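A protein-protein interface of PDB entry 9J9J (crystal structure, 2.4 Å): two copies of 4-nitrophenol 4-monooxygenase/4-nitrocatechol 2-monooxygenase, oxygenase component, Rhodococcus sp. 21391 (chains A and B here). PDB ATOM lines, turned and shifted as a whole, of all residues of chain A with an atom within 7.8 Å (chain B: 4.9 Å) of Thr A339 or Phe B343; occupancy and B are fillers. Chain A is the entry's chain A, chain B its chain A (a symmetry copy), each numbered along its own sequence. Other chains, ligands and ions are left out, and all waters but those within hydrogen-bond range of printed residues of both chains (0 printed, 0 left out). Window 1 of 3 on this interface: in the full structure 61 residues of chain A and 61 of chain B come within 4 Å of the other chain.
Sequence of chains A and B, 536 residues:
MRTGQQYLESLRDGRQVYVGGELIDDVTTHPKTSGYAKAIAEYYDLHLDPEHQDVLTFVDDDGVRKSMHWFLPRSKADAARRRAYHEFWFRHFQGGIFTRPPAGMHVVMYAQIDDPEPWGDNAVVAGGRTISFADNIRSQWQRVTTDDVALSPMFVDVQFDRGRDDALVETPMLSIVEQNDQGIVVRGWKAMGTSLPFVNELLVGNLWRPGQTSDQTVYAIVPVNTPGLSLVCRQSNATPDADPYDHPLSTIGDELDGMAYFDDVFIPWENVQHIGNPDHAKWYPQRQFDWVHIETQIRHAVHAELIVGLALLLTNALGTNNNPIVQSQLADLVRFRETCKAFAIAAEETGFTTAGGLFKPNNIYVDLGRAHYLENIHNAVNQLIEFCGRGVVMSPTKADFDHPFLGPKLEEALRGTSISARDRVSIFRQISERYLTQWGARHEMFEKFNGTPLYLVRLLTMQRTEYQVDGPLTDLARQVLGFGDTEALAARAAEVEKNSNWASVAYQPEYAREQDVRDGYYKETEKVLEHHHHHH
The side-chain carboxylate (OE1) of Glu A338 is in hydrogen-bond range of the side-chain hydroxyl (OH) of Tyr B365 (3.3 Å).
OE2 of Glu A338 lies within salt-bridge range of NH1 of Arg A337.
The guanidinium group of Arg A335 is in salt-bridge range of the side-chain carboxylate of Asp A332.
The backbone carbonyl oxygen of Arg A335 sits at hydrogen-bond distance from the side-chain hydroxyl of Thr A339.
Arg A335 touches Leu B368 (CD to O, 3.6 Å).
CG of Glu A338 touches CD1 of Leu B368 (3.6 Å).
OG1 of Thr A339 touches CZ of Phe B343, 3.4 Å away.
CG of Lys A341 touches OH of Tyr B365, 3.5 Å away.
CB of Ala A342 touches CB of Ala B346 (3.8 Å).
Phe A343 touches Thr B339 (CZ to OG1, 3.4 Å).
CD1 of Ile A345 touches OH of Tyr B365 (3.8 Å).
CB of Ala A346 touches CB of Ala B342, at 3.8 Å.
Lys B341 touches Tyr A365.
Tyr A365 touches Ile B345.
Leu A333 touches none of the printed residues of chain B.
Thr A339 touches just one residue of chain B: Phe B343 (3.4 Å).
Printed residues of chain B within 4 Å of Lys A341: Tyr B365 (3.5 Å).
Of the printed residues of chain B, Ala A342 touches Ala B346 (3.8 Å).
Ala B342 touches just one residue of chain A: Ala A346.
Of chain A, only Thr A339 comes within 4 Å of Phe B343.
No residue of chain A comes within 4 Å of Ala B344.
The nearest residue of chain B that does not touch Thr A339 is Thr B339 (4.1 Å).
The nearest printed residue of chain A that does not touch Phe B343 is Glu A338 (4.1 Å).
Hydrophobic or aromatic side chains of chain B within 4 Å of the printed part of chain A: Ala B342, Phe B343, Ile B345, Ala B346, Tyr B365 and Leu B368.
Along chain B the printed residues that touch a printed residue of chain A span positions 339 to 368.
Hydrophobic or aromatic side chains of chain A within 4 Å of the printed part of chain B: Ala A342, Phe A343, Ile A345, Ala A346 and Tyr A365.
Among the printed residues, 11 pairs touch across the chains.
Among the printed residues, no Asp or Glu carboxylate lies within 4 Å of a Lys or Arg side-chain nitrogen of the other chain.
Thr A339 touches Phe B343, and with the chains exchanged Phe A343 touches Thr B339.
Lys A341 touches Tyr B365, and with the chains exchanged Tyr A365 touches Lys B341.
Ala A342 touches Ala B346, and with the chains exchanged Ala A346 touches Ala B342.
Ile A345 touches Tyr B365, and with the chains exchanged Tyr A365 touches Ile B345.
13 positions are printed for both chains.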
ATOM      1  N   GLN A 297      22.737  -7.016 -17.677  1.00  0.00           N
ATOM      2  CA  GLN A 297      21.479  -7.740 -17.775  1.00  0.00           C
ATOM      3  C   GLN A 297      21.144  -7.989 -19.239  1.00  0.00           C
ATOM      4  O   GLN A 297      20.514  -8.991 -19.584  1.00  0.00           O
ATOM      5  CB  GLN A 297      20.337  -6.959 -17.132  1.00  0.00           C
ATOM      6  CG  GLN A 297      19.116  -7.790 -16.742  1.00  0.00           C
ATOM      7  CD  GLN A 297      18.104  -7.877 -17.850  1.00  0.00           C
ATOM      8  OE1 GLN A 297      17.849  -6.878 -18.512  1.00  0.00           O
ATOM      9  NE2 GLN A 297      17.539  -9.058 -18.081  1.00  0.00           N
ATOM     10  N   ALA A 301      20.891 -11.959 -21.295  1.00  0.00           N
ATOM     11  CA  ALA A 301      19.916 -12.456 -22.237  1.00  0.00           C
ATOM     12  C   ALA A 301      20.622 -13.012 -23.462  1.00  0.00           C
ATOM     13  O   ALA A 301      20.185 -13.999 -24.049  1.00  0.00           O
ATOM     14  CB  ALA A 301      18.955 -11.367 -22.597  1.00  0.00           C
ATOM     15  N   ALA A 304      22.155 -16.461 -22.539  1.00  0.00           N
ATOM     16  CA  ALA A 304      21.070 -17.439 -22.582  1.00  0.00           C
ATOM     17  C   ALA A 304      20.675 -17.743 -24.026  1.00  0.00           C
ATOM     18  O   ALA A 304      20.456 -18.888 -24.399  1.00  0.00           O
ATOM     19  CB  ALA A 304      19.878 -16.938 -21.759  1.00  0.00           C
ATOM     20  N   ASP A 332      12.612 -25.253 -21.428  1.00  0.00           N
ATOM     21  CA  ASP A 332      12.979 -24.483 -20.249  1.00  0.00           C
ATOM     22  C   ASP A 332      14.230 -23.644 -20.518  1.00  0.00           C
ATOM     23  O   ASP A 332      14.372 -22.536 -19.997  1.00  0.00           O
ATOM     24  CB  ASP A 332      13.104 -25.343 -18.989  1.00  0.00           C
ATOM     25  CG  ASP A 332      11.800 -25.841 -18.349  1.00  0.00           C
ATOM     26  OD1 ASP A 332      10.692 -25.388 -18.717  1.00  0.00           O
ATOM     27  OD2 ASP A 332      11.888 -26.739 -17.519  1.00  0.00           O
ATOM     28  N   LEU A 333      15.132 -24.105 -21.382  1.00  0.00           N
ATOM     29  CA  LEU A 333      16.203 -23.203 -21.769  1.00  0.00           C
ATOM     30  C   LEU A 333      15.647 -22.031 -22.569  1.00  0.00           C
ATOM     31  O   LEU A 333      16.082 -20.895 -22.426  1.00  0.00           O
ATOM     32  CB  LEU A 333      17.274 -23.951 -22.542  1.00  0.00           C
ATOM     33  CG  LEU A 333      18.098 -24.934 -21.725  1.00  0.00           C
ATOM     34  CD1 LEU A 333      19.078 -25.662 -22.613  1.00  0.00           C
ATOM     35  CD2 LEU A 333      18.794 -24.242 -20.596  1.00  0.00           C
ATOM     36  N   VAL A 334      14.651 -22.285 -23.412  1.00  0.00           N
ATOM     37  CA  VAL A 334      14.079 -21.187 -24.172  1.00  0.00           C
ATOM     38  C   VAL A 334      13.449 -20.196 -23.210  1.00  0.00           C
ATOM     39  O   VAL A 334      13.667 -18.999 -23.325  1.00  0.00           O
ATOM     40  CB  VAL A 334      13.054 -21.703 -25.185  1.00  0.00           C
ATOM     41  CG1 VAL A 334      12.230 -20.563 -25.764  1.00  0.00           C
ATOM     42  CG2 VAL A 334      13.737 -22.494 -26.274  1.00  0.00           C
ATOM     43  N   ARG A 335      12.734 -20.722 -22.209  1.00  0.00           N
ATOM     44  CA  ARG A 335      12.063 -19.893 -21.221  1.00  0.00           C
ATOM     45  C   ARG A 335      13.069 -19.114 -20.402  1.00  0.00           C
ATOM     46  O   ARG A 335      12.797 -17.979 -20.011  1.00  0.00           O
ATOM     47  CB  ARG A 335      11.125 -20.677 -20.311  1.00  0.00           C
ATOM     48  CG  ARG A 335      10.446 -19.768 -19.297  1.00  0.00           C
ATOM     49  CD  ARG A 335       9.165 -20.347 -18.770  1.00  0.00           C
ATOM     50  NE  ARG A 335       9.374 -21.761 -18.431  1.00  0.00           N
ATOM     51  CZ  ARG A 335       9.595 -22.177 -17.202  1.00  0.00           C
ATOM     52  NH1 ARG A 335       9.799 -21.297 -16.252  1.00  0.00           N
ATOM     53  NH2 ARG A 335       9.647 -23.463 -16.933  1.00  0.00           N
ATOM     54  N   PHE A 336      14.239 -19.693 -20.155  1.00  0.00           N
ATOM     55  CA  PHE A 336      15.269 -18.952 -19.424  1.00  0.00           C
ATOM     56  C   PHE A 336      15.702 -17.733 -20.245  1.00  0.00           C
ATOM     57  O   PHE A 336      15.782 -16.626 -19.747  1.00  0.00           O
ATOM     58  CB  PHE A 336      16.382 -19.942 -19.092  1.00  0.00           C
ATOM     59  CG  PHE A 336      17.571 -19.299 -18.411  1.00  0.00           C
ATOM     60  CD1 PHE A 336      17.466 -18.812 -17.116  1.00  0.00           C
ATOM     61  CD2 PHE A 336      18.799 -19.226 -19.052  1.00  0.00           C
ATOM     62  CE1 PHE A 336      18.546 -18.220 -16.498  1.00  0.00           C
ATOM     63  CE2 PHE A 336      19.865 -18.612 -18.430  1.00  0.00           C
ATOM     64  CZ  PHE A 336      19.744 -18.128 -17.146  1.00  0.00           C
ATOM     65  N   ARG A 337      15.875 -17.916 -21.549  1.00  0.00           N
ATOM     66  CA  ARG A 337      16.235 -16.820 -22.413  1.00  0.00           C
ATOM     67  C   ARG A 337      15.142 -15.779 -22.429  1.00  0.00           C
ATOM     68  O   ARG A 337      15.411 -14.568 -22.292  1.00  0.00           O
ATOM     69  CB  ARG A 337      16.516 -17.338 -23.823  1.00  0.00           C
ATOM     70  CG  ARG A 337      17.030 -16.282 -24.793  1.00  0.00           C
ATOM     71  CD  ARG A 337      15.930 -15.675 -25.567  1.00  0.00           C
ATOM     72  NE  ARG A 337      16.448 -14.708 -26.523  1.00  0.00           N
ATOM     73  CZ  ARG A 337      16.033 -14.570 -27.789  1.00  0.00           C
ATOM     74  NH1 ARG A 337      14.983 -15.242 -28.245  1.00  0.00           N
ATOM     75  NH2 ARG A 337      16.692 -13.750 -28.604  1.00  0.00           N
ATOM     76  N   GLU A 338      13.911 -16.224 -22.625  1.00  0.00           N
ATOM     77  CA  GLU A 338      12.856 -15.232 -22.819  1.00  0.00           C
ATOM     78  C   GLU A 338      12.556 -14.473 -21.530  1.00  0.00           C
ATOM     79  O   GLU A 338      12.140 -13.318 -21.591  1.00  0.00           O
ATOM     80  CB  GLU A 338      11.585 -15.809 -23.439  1.00  0.00           C
ATOM     81  CG  GLU A 338      11.815 -16.423 -24.808  1.00  0.00           C
ATOM     82  CD  GLU A 338      12.193 -15.432 -25.884  1.00  0.00           C
ATOM     83  OE1 GLU A 338      12.170 -14.217 -25.595  1.00  0.00           O
ATOM     84  OE2 GLU A 338      12.449 -15.894 -27.021  1.00  0.00           O
ATOM     85  N   THR A 339      12.782 -15.088 -20.368  1.00  0.00           N
ATOM     86  CA  THR A 339      12.663 -14.390 -19.097  1.00  0.00           C
ATOM     87  C   THR A 339      13.645 -13.225 -19.030  1.00  0.00           C
ATOM     88  O   THR A 339      13.283 -12.099 -18.699  1.00  0.00           O
ATOM     89  CB  THR A 339      12.857 -15.370 -17.929  1.00  0.00           C
ATOM     90  OG1 THR A 339      11.900 -16.412 -18.061  1.00  0.00           O
ATOM     91  CG2 THR A 339      12.470 -14.748 -16.606  1.00  0.00           C
ATOM     92  N   CYS A 340      14.916 -13.473 -19.320  1.00  0.00           N
ATOM     93  CA  CYS A 340      15.908 -12.404 -19.280  1.00  0.00           C
ATOM     94  C   CYS A 340      15.536 -11.312 -20.279  1.00  0.00           C
ATOM     95  O   CYS A 340      15.493 -10.126 -19.967  1.00  0.00           O
ATOM     96  CB  CYS A 340      17.292 -12.955 -19.581  1.00  0.00           C
ATOM     97  SG  CYS A 340      17.890 -14.140 -18.352  1.00  0.00           S
ATOM     98  N   LYS A 341      15.134 -11.725 -21.474  1.00  0.00           N
ATOM     99  CA  LYS A 341      14.747 -10.745 -22.478  1.00  0.00           C
ATOM    100  C   LYS A 341      13.556  -9.900 -22.007  1.00  0.00           C
ATOM    101  O   LYS A 341      13.550  -8.681 -22.173  1.00  0.00           O
ATOM    102  CB  LYS A 341      14.552 -11.496 -23.793  1.00  0.00           C
ATOM    103  CG  LYS A 341      14.297 -10.603 -24.960  1.00  0.00           C
ATOM    104  CD  LYS A 341      14.526 -11.297 -26.282  1.00  0.00           C
ATOM    105  CE  LYS A 341      14.217 -10.303 -27.351  1.00  0.00           C
ATOM    106  NZ  LYS A 341      13.932 -11.092 -28.544  1.00  0.00           N
ATOM    107  N   ALA A 342      12.556 -10.533 -21.385  1.00  0.00           N
ATOM    108  CA  ALA A 342      11.378  -9.805 -20.917  1.00  0.00           C
ATOM    109  C   ALA A 342      11.727  -8.794 -19.835  1.00  0.00           C
ATOM    110  O   ALA A 342      11.126  -7.719 -19.792  1.00  0.00           O
ATOM    111  CB  ALA A 342      10.315 -10.749 -20.403  1.00  0.00           C
ATOM    112  N   PHE A 343      12.643  -9.142 -18.913  1.00  0.00           N
ATOM    113  CA  PHE A 343      13.012  -8.168 -17.910  1.00  0.00           C
ATOM    114  C   PHE A 343      13.709  -6.975 -18.573  1.00  0.00           C
ATOM    115  O   PHE A 343      13.485  -5.832 -18.198  1.00  0.00           O
ATOM    116  CB  PHE A 343      13.903  -8.784 -16.844  1.00  0.00           C
ATOM    117  CG  PHE A 343      13.182  -9.383 -15.663  1.00  0.00           C
ATOM    118  CD1 PHE A 343      12.600  -8.566 -14.710  1.00  0.00           C
ATOM    119  CD2 PHE A 343      13.063 -10.751 -15.526  1.00  0.00           C
ATOM    120  CE1 PHE A 343      11.959  -9.119 -13.618  1.00  0.00           C
ATOM    121  CE2 PHE A 343      12.451 -11.292 -14.414  1.00  0.00           C
ATOM    122  CZ  PHE A 343      11.906 -10.486 -13.469  1.00  0.00           C
ATOM    123  N   ALA A 344      14.549  -7.225 -19.575  1.00  0.00           N
ATOM    124  CA  ALA A 344      15.204  -6.140 -20.294  1.00  0.00           C
ATOM    125  C   ALA A 344      14.198  -5.230 -20.991  1.00  0.00           C
ATOM    126  O   ALA A 344      14.327  -4.005 -20.928  1.00  0.00           O
ATOM    127  CB  ALA A 344      16.180  -6.697 -21.289  1.00  0.00           C
ATOM    128  N   ILE A 345      13.189  -5.814 -21.625  1.00  0.00           N
ATOM    129  CA  ILE A 345      12.141  -5.018 -22.256  1.00  0.00           C
ATOM    130  C   ILE A 345      11.334  -4.258 -21.213  1.00  0.00           C
ATOM    131  O   ILE A 345      11.037  -3.074 -21.392  1.00  0.00           O
ATOM    132  CB  ILE A 345      11.244  -5.880 -23.140  1.00  0.00           C
ATOM    133  CG1 ILE A 345      11.992  -6.315 -24.378  1.00  0.00           C
ATOM    134  CG2 ILE A 345       9.972  -5.129 -23.501  1.00  0.00           C
ATOM    135  CD1 ILE A 345      11.404  -7.529 -25.051  1.00  0.00           C
ATOM    136  N   ALA A 346      10.997  -4.904 -20.095  1.00  0.00           N
ATOM    137  CA  ALA A 346      10.174  -4.219 -19.108  1.00  0.00           C
ATOM    138  C   ALA A 346      10.950  -3.070 -18.483  1.00  0.00           C
ATOM    139  O   ALA A 346      10.376  -2.047 -18.103  1.00  0.00           O
ATOM    140  CB  ALA A 346       9.689  -5.181 -18.063  1.00  0.00           C
ATOM    141  N   TYR A 365      13.260  -3.841 -12.672  1.00  0.00           N
ATOM    142  CA  TYR A 365      13.310  -4.926 -13.623  1.00  0.00           C
ATOM    143  C   TYR A 365      14.741  -5.291 -13.961  1.00  0.00           C
ATOM    144  O   TYR A 365      15.021  -6.463 -14.187  1.00  0.00           O
ATOM    145  CB  TYR A 365      12.500  -4.563 -14.857  1.00  0.00           C
ATOM    146  CG  TYR A 365      11.036  -4.438 -14.489  1.00  0.00           C
ATOM    147  CD1 TYR A 365      10.303  -5.549 -14.101  1.00  0.00           C
ATOM    148  CD2 TYR A 365      10.412  -3.204 -14.485  1.00  0.00           C
ATOM    149  CE1 TYR A 365       8.970  -5.432 -13.747  1.00  0.00           C
ATOM    150  CE2 TYR A 365       9.068  -3.084 -14.186  1.00  0.00           C
ATOM    151  CZ  TYR A 365       8.351  -4.198 -13.798  1.00  0.00           C
ATOM    152  OH  TYR A 365       7.043  -4.038 -13.475  1.00  0.00           O
ATOM    153  N   LEU A 368      15.944  -7.472 -10.850  1.00  0.00           N
ATOM    154  CA  LEU A 368      15.220  -8.697 -10.659  1.00  0.00           C
ATOM    155  C   LEU A 368      15.495  -9.609 -11.838  1.00  0.00           C
ATOM    156  O   LEU A 368      15.554 -10.794 -11.634  1.00  0.00           O
ATOM    157  CB  LEU A 368      13.746  -8.495 -10.318  1.00  0.00           C
ATOM    158  CG  LEU A 368      13.527  -7.697  -9.025  1.00  0.00           C
ATOM    159  CD1 LEU A 368      12.063  -7.551  -8.687  1.00  0.00           C
ATOM    160  CD2 LEU A 368      14.246  -8.284  -7.850  1.00  0.00           C
ATOM    161  N   GLY A 369      15.777  -9.063 -13.010  1.00  0.00           N
ATOM    162  CA  GLY A 369      16.208  -9.851 -14.147  1.00  0.00           C
ATOM    163  C   GLY A 369      17.591 -10.438 -13.908  1.00  0.00           C
ATOM    164  O   GLY A 369      17.856 -11.622 -14.159  1.00  0.00           O
ATOM    165  N   HIS A 372      17.190 -13.326 -11.605  1.00  0.00           N
ATOM    166  CA  HIS A 372      16.663 -14.505 -12.277  1.00  0.00           C
ATOM    167  C   HIS A 372      17.791 -15.264 -12.972  1.00  0.00           C
ATOM    168  O   HIS A 372      17.820 -16.485 -12.929  1.00  0.00           O
ATOM    169  CB  HIS A 372      15.625 -14.141 -13.335  1.00  0.00           C
ATOM    170  CG  HIS A 372      15.013 -15.369 -13.910  1.00  0.00           C
ATOM    171  ND1 HIS A 372      15.477 -16.033 -15.024  1.00  0.00           N
ATOM    172  CD2 HIS A 372      14.001 -16.097 -13.438  1.00  0.00           C
ATOM    173  CE1 HIS A 372      14.728 -17.103 -15.217  1.00  0.00           C
ATOM    174  NE2 HIS A 372      13.831 -17.154 -14.267  1.00  0.00           N
ATOM    175  N   TYR A 373      18.653 -14.521 -13.670  1.00  0.00           N
ATOM    176  CA  TYR A 373      19.852 -15.070 -14.274  1.00  0.00           C
ATOM    177  C   TYR A 373      20.726 -15.685 -13.199  1.00  0.00           C
ATOM    178  O   TYR A 373      21.110 -16.836 -13.311  1.00  0.00           O
ATOM    179  CB  TYR A 373      20.674 -14.025 -15.039  1.00  0.00           C
ATOM    180  CG  TYR A 373      21.942 -14.508 -15.732  1.00  0.00           C
ATOM    181  CD1 TYR A 373      23.171 -14.532 -15.091  1.00  0.00           C
ATOM    182  CD2 TYR A 373      21.907 -15.001 -17.020  1.00  0.00           C
ATOM    183  CE1 TYR A 373      24.325 -14.994 -15.704  1.00  0.00           C
ATOM    184  CE2 TYR A 373      23.062 -15.409 -17.671  1.00  0.00           C
ATOM    185  CZ  TYR A 373      24.277 -15.403 -17.015  1.00  0.00           C
ATOM    186  OH  TYR A 373      25.382 -15.867 -17.672  1.00  0.00           O
ATOM    187  N   ASN A 376      19.558 -19.138 -11.683  1.00  0.00           N
ATOM    188  CA  ASN A 376      19.281 -20.271 -12.530  1.00  0.00           C
ATOM    189  C   ASN A 376      20.414 -20.587 -13.521  1.00  0.00           C
ATOM    190  O   ASN A 376      20.389 -21.660 -14.109  1.00  0.00           O
ATOM    191  CB  ASN A 376      17.968 -20.048 -13.271  1.00  0.00           C
ATOM    192  CG  ASN A 376      16.801 -19.967 -12.320  1.00  0.00           C
ATOM    193  OD1 ASN A 376      16.414 -20.973 -11.728  1.00  0.00           O
ATOM    194  ND2 ASN A 376      16.246 -18.783 -12.132  1.00  0.00           N
ATOM    195  N   GLN B 297      -2.962 -14.362 -17.745  1.00  0.00           N
ATOM    196  CA  GLN B 297      -1.591 -14.038 -17.384  1.00  0.00           C
ATOM    197  C   GLN B 297      -1.559 -12.720 -16.622  1.00  0.00           C
ATOM    198  O   GLN B 297      -0.705 -12.507 -15.758  1.00  0.00           O
ATOM    199  CB  GLN B 297      -0.706 -13.915 -18.620  1.00  0.00           C
ATOM    200  CG  GLN B 297       0.793 -14.063 -18.368  1.00  0.00           C
ATOM    201  CD  GLN B 297       1.457 -12.748 -18.066  1.00  0.00           C
ATOM    202  OE1 GLN B 297       1.145 -11.754 -18.712  1.00  0.00           O
ATOM    203  NE2 GLN B 297       2.348 -12.717 -17.080  1.00  0.00           N
ATOM    204  N   THR B 339       8.299 -10.889 -12.033  1.00  0.00           N
ATOM    205  CA  THR B 339       8.457 -11.723 -13.216  1.00  0.00           C
ATOM    206  C   THR B 339       7.158 -11.774 -14.014  1.00  0.00           C
ATOM    207  O   THR B 339       7.140 -11.562 -15.224  1.00  0.00           O
ATOM    208  CB  THR B 339       8.940 -13.127 -12.818  1.00  0.00           C
ATOM    209  OG1 THR B 339      10.154 -12.989 -12.092  1.00  0.00           O
ATOM    210  CG2 THR B 339       9.378 -13.930 -14.022  1.00  0.00           C
ATOM    211  N   CYS B 340       6.045 -12.080 -13.360  1.00  0.00           N
ATOM    212  CA  CYS B 340       4.767 -12.143 -14.061  1.00  0.00           C
ATOM    213  C   CYS B 340       4.442 -10.782 -14.672  1.00  0.00           C
ATOM    214  O   CYS B 340       4.111 -10.654 -15.847  1.00  0.00           O
ATOM    215  CB  CYS B 340       3.663 -12.579 -13.112  1.00  0.00           C
ATOM    216  SG  CYS B 340       3.878 -14.254 -12.463  1.00  0.00           S
ATOM    217  N   LYS B 341       4.662  -9.726 -13.899  1.00  0.00           N
ATOM    218  CA  LYS B 341       4.391  -8.393 -14.414  1.00  0.00           C
ATOM    219  C   LYS B 341       5.254  -8.081 -15.645  1.00  0.00           C
ATOM    220  O   LYS B 341       4.760  -7.541 -16.634  1.00  0.00           O
ATOM    221  CB  LYS B 341       4.523  -7.419 -13.245  1.00  0.00           C
ATOM    222  CG  LYS B 341       4.127  -6.022 -13.583  1.00  0.00           C
ATOM    223  CD  LYS B 341       3.858  -5.184 -12.356  1.00  0.00           C
ATOM    224  CE  LYS B 341       3.496  -3.818 -12.836  1.00  0.00           C
ATOM    225  NZ  LYS B 341       3.753  -2.930 -11.708  1.00  0.00           N
ATOM    226  N   ALA B 342       6.539  -8.450 -15.609  1.00  0.00           N
ATOM    227  CA  ALA B 342       7.432  -8.179 -16.733  1.00  0.00           C
ATOM    228  C   ALA B 342       7.008  -8.924 -17.990  1.00  0.00           C
ATOM    229  O   ALA B 342       7.151  -8.388 -19.091  1.00  0.00           O
ATOM    230  CB  ALA B 342       8.864  -8.531 -16.396  1.00  0.00           C
ATOM    231  N   PHE B 343       6.548 -10.181 -17.858  1.00  0.00           N
ATOM    232  CA  PHE B 343       6.100 -10.876 -19.044  1.00  0.00           C
ATOM    233  C   PHE B 343       4.865 -10.177 -19.623  1.00  0.00           C
ATOM    234  O   PHE B 343       4.728 -10.050 -20.832  1.00  0.00           O
ATOM    235  CB  PHE B 343       5.798 -12.336 -18.746  1.00  0.00           C
ATOM    236  CG  PHE B 343       6.959 -13.284 -18.912  1.00  0.00           C
ATOM    237  CD1 PHE B 343       7.407 -13.629 -20.174  1.00  0.00           C
ATOM    238  CD2 PHE B 343       7.613 -13.800 -17.812  1.00  0.00           C
ATOM    239  CE1 PHE B 343       8.457 -14.515 -20.322  1.00  0.00           C
ATOM    240  CE2 PHE B 343       8.638 -14.711 -17.971  1.00  0.00           C
ATOM    241  CZ  PHE B 343       9.055 -15.067 -19.211  1.00  0.00           C
ATOM    242  N   ALA B 344       3.962  -9.703 -18.769  1.00  0.00           N
ATOM    243  CA  ALA B 344       2.792  -8.975 -19.240  1.00  0.00           C
ATOM    244  C   ALA B 344       3.176  -7.697 -19.980  1.00  0.00           C
ATOM    245  O   ALA B 344       2.616  -7.405 -21.039  1.00  0.00           O
ATOM    246  CB  ALA B 344       1.884  -8.657 -18.088  1.00  0.00           C
ATOM    247  N   ILE B 345       4.140  -6.955 -19.449  1.00  0.00           N
ATOM    248  CA  ILE B 345       4.621  -5.757 -20.128  1.00  0.00           C
ATOM    249  C   ILE B 345       5.314  -6.114 -21.435  1.00  0.00           C
ATOM    250  O   ILE B 345       5.091  -5.465 -22.460  1.00  0.00           O
ATOM    251  CB  ILE B 345       5.529  -4.930 -19.220  1.00  0.00           C
ATOM    252  CG1 ILE B 345       4.719  -4.276 -18.126  1.00  0.00           C
ATOM    253  CG2 ILE B 345       6.294  -3.896 -20.031  1.00  0.00           C
ATOM    254  CD1 ILE B 345       5.534  -3.863 -16.928  1.00  0.00           C
ATOM    255  N   ALA B 346       6.133  -7.168 -21.438  1.00  0.00           N
ATOM    256  CA  ALA B 346       6.855  -7.494 -22.660  1.00  0.00           C
ATOM    257  C   ALA B 346       5.884  -7.958 -23.735  1.00  0.00           C
ATOM    258  O   ALA B 346       6.106  -7.742 -24.928  1.00  0.00           O
ATOM    259  CB  ALA B 346       7.908  -8.530 -22.393  1.00  0.00           C
ATOM    260  N   ALA B 347       4.817  -8.637 -23.305  1.00  0.00           N
ATOM    261  CA  ALA B 347       3.849  -9.149 -24.249  1.00  0.00           C
ATOM    262  C   ALA B 347       3.141  -7.988 -24.938  1.00  0.00           C
ATOM    263  O   ALA B 347       2.993  -7.980 -26.147  1.00  0.00           O
ATOM    264  CB  ALA B 347       2.874 -10.045 -23.560  1.00  0.00           C
ATOM    265  N   TYR B 365       5.545 -14.122 -24.992  1.00  0.00           N
ATOM    266  CA  TYR B 365       5.673 -13.666 -23.628  1.00  0.00           C
ATOM    267  C   TYR B 365       4.448 -14.027 -22.813  1.00  0.00           C
ATOM    268  O   TYR B 365       4.583 -14.314 -21.628  1.00  0.00           O
ATOM    269  CB  TYR B 365       5.956 -12.172 -23.614  1.00  0.00           C
ATOM    270  CG  TYR B 365       7.307 -11.901 -24.241  1.00  0.00           C
ATOM    271  CD1 TYR B 365       8.475 -12.321 -23.624  1.00  0.00           C
ATOM    272  CD2 TYR B 365       7.402 -11.272 -25.469  1.00  0.00           C
ATOM    273  CE1 TYR B 365       9.709 -12.089 -24.207  1.00  0.00           C
ATOM    274  CE2 TYR B 365       8.631 -10.988 -26.033  1.00  0.00           C
ATOM    275  CZ  TYR B 365       9.786 -11.415 -25.409  1.00  0.00           C
ATOM    276  OH  TYR B 365      10.973 -11.152 -26.010  1.00  0.00           O
ATOM    277  N   LEU B 368       4.961 -17.886 -21.958  1.00  0.00           N
ATOM    278  CA  LEU B 368       6.115 -18.176 -21.155  1.00  0.00           C
ATOM    279  C   LEU B 368       5.922 -17.549 -19.788  1.00  0.00           C
ATOM    280  O   LEU B 368       6.365 -18.131 -18.832  1.00  0.00           O
ATOM    281  CB  LEU B 368       7.441 -17.852 -21.840  1.00  0.00           C
ATOM    282  CG  LEU B 368       7.655 -18.635 -23.144  1.00  0.00           C
ATOM    283  CD1 LEU B 368       8.992 -18.331 -23.777  1.00  0.00           C
ATOM    284  CD2 LEU B 368       7.523 -20.115 -22.961  1.00  0.00           C
ATOM    285  N   GLY B 369       5.175 -16.461 -19.689  1.00  0.00           N
ATOM    286  CA  GLY B 369       4.806 -15.889 -18.410  1.00  0.00           C
ATOM    287  C   GLY B 369       3.851 -16.807 -17.662  1.00  0.00           C
ATOM    288  O   GLY B 369       3.997 -17.070 -16.460  1.00  0.00           O
ATOM    289  N   HIS B 372       5.863 -19.589 -16.242  1.00  0.00           N
ATOM    290  CA  HIS B 372       6.611 -19.187 -15.059  1.00  0.00           C
ATOM    291  C   HIS B 372       5.716 -19.252 -13.823  1.00  0.00           C
ATOM    292  O   HIS B 372       6.160 -19.695 -12.773  1.00  0.00           O
ATOM    293  CB  HIS B 372       7.139 -17.761 -15.177  1.00  0.00           C
ATOM    294  CG  HIS B 372       8.006 -17.428 -14.014  1.00  0.00           C
ATOM    295  ND1 HIS B 372       7.566 -16.849 -12.844  1.00  0.00           N
ATOM    296  CD2 HIS B 372       9.300 -17.692 -13.834  1.00  0.00           C
ATOM    297  CE1 HIS B 372       8.589 -16.745 -12.016  1.00  0.00           C
ATOM    298  NE2 HIS B 372       9.644 -17.250 -12.602  1.00  0.00           N
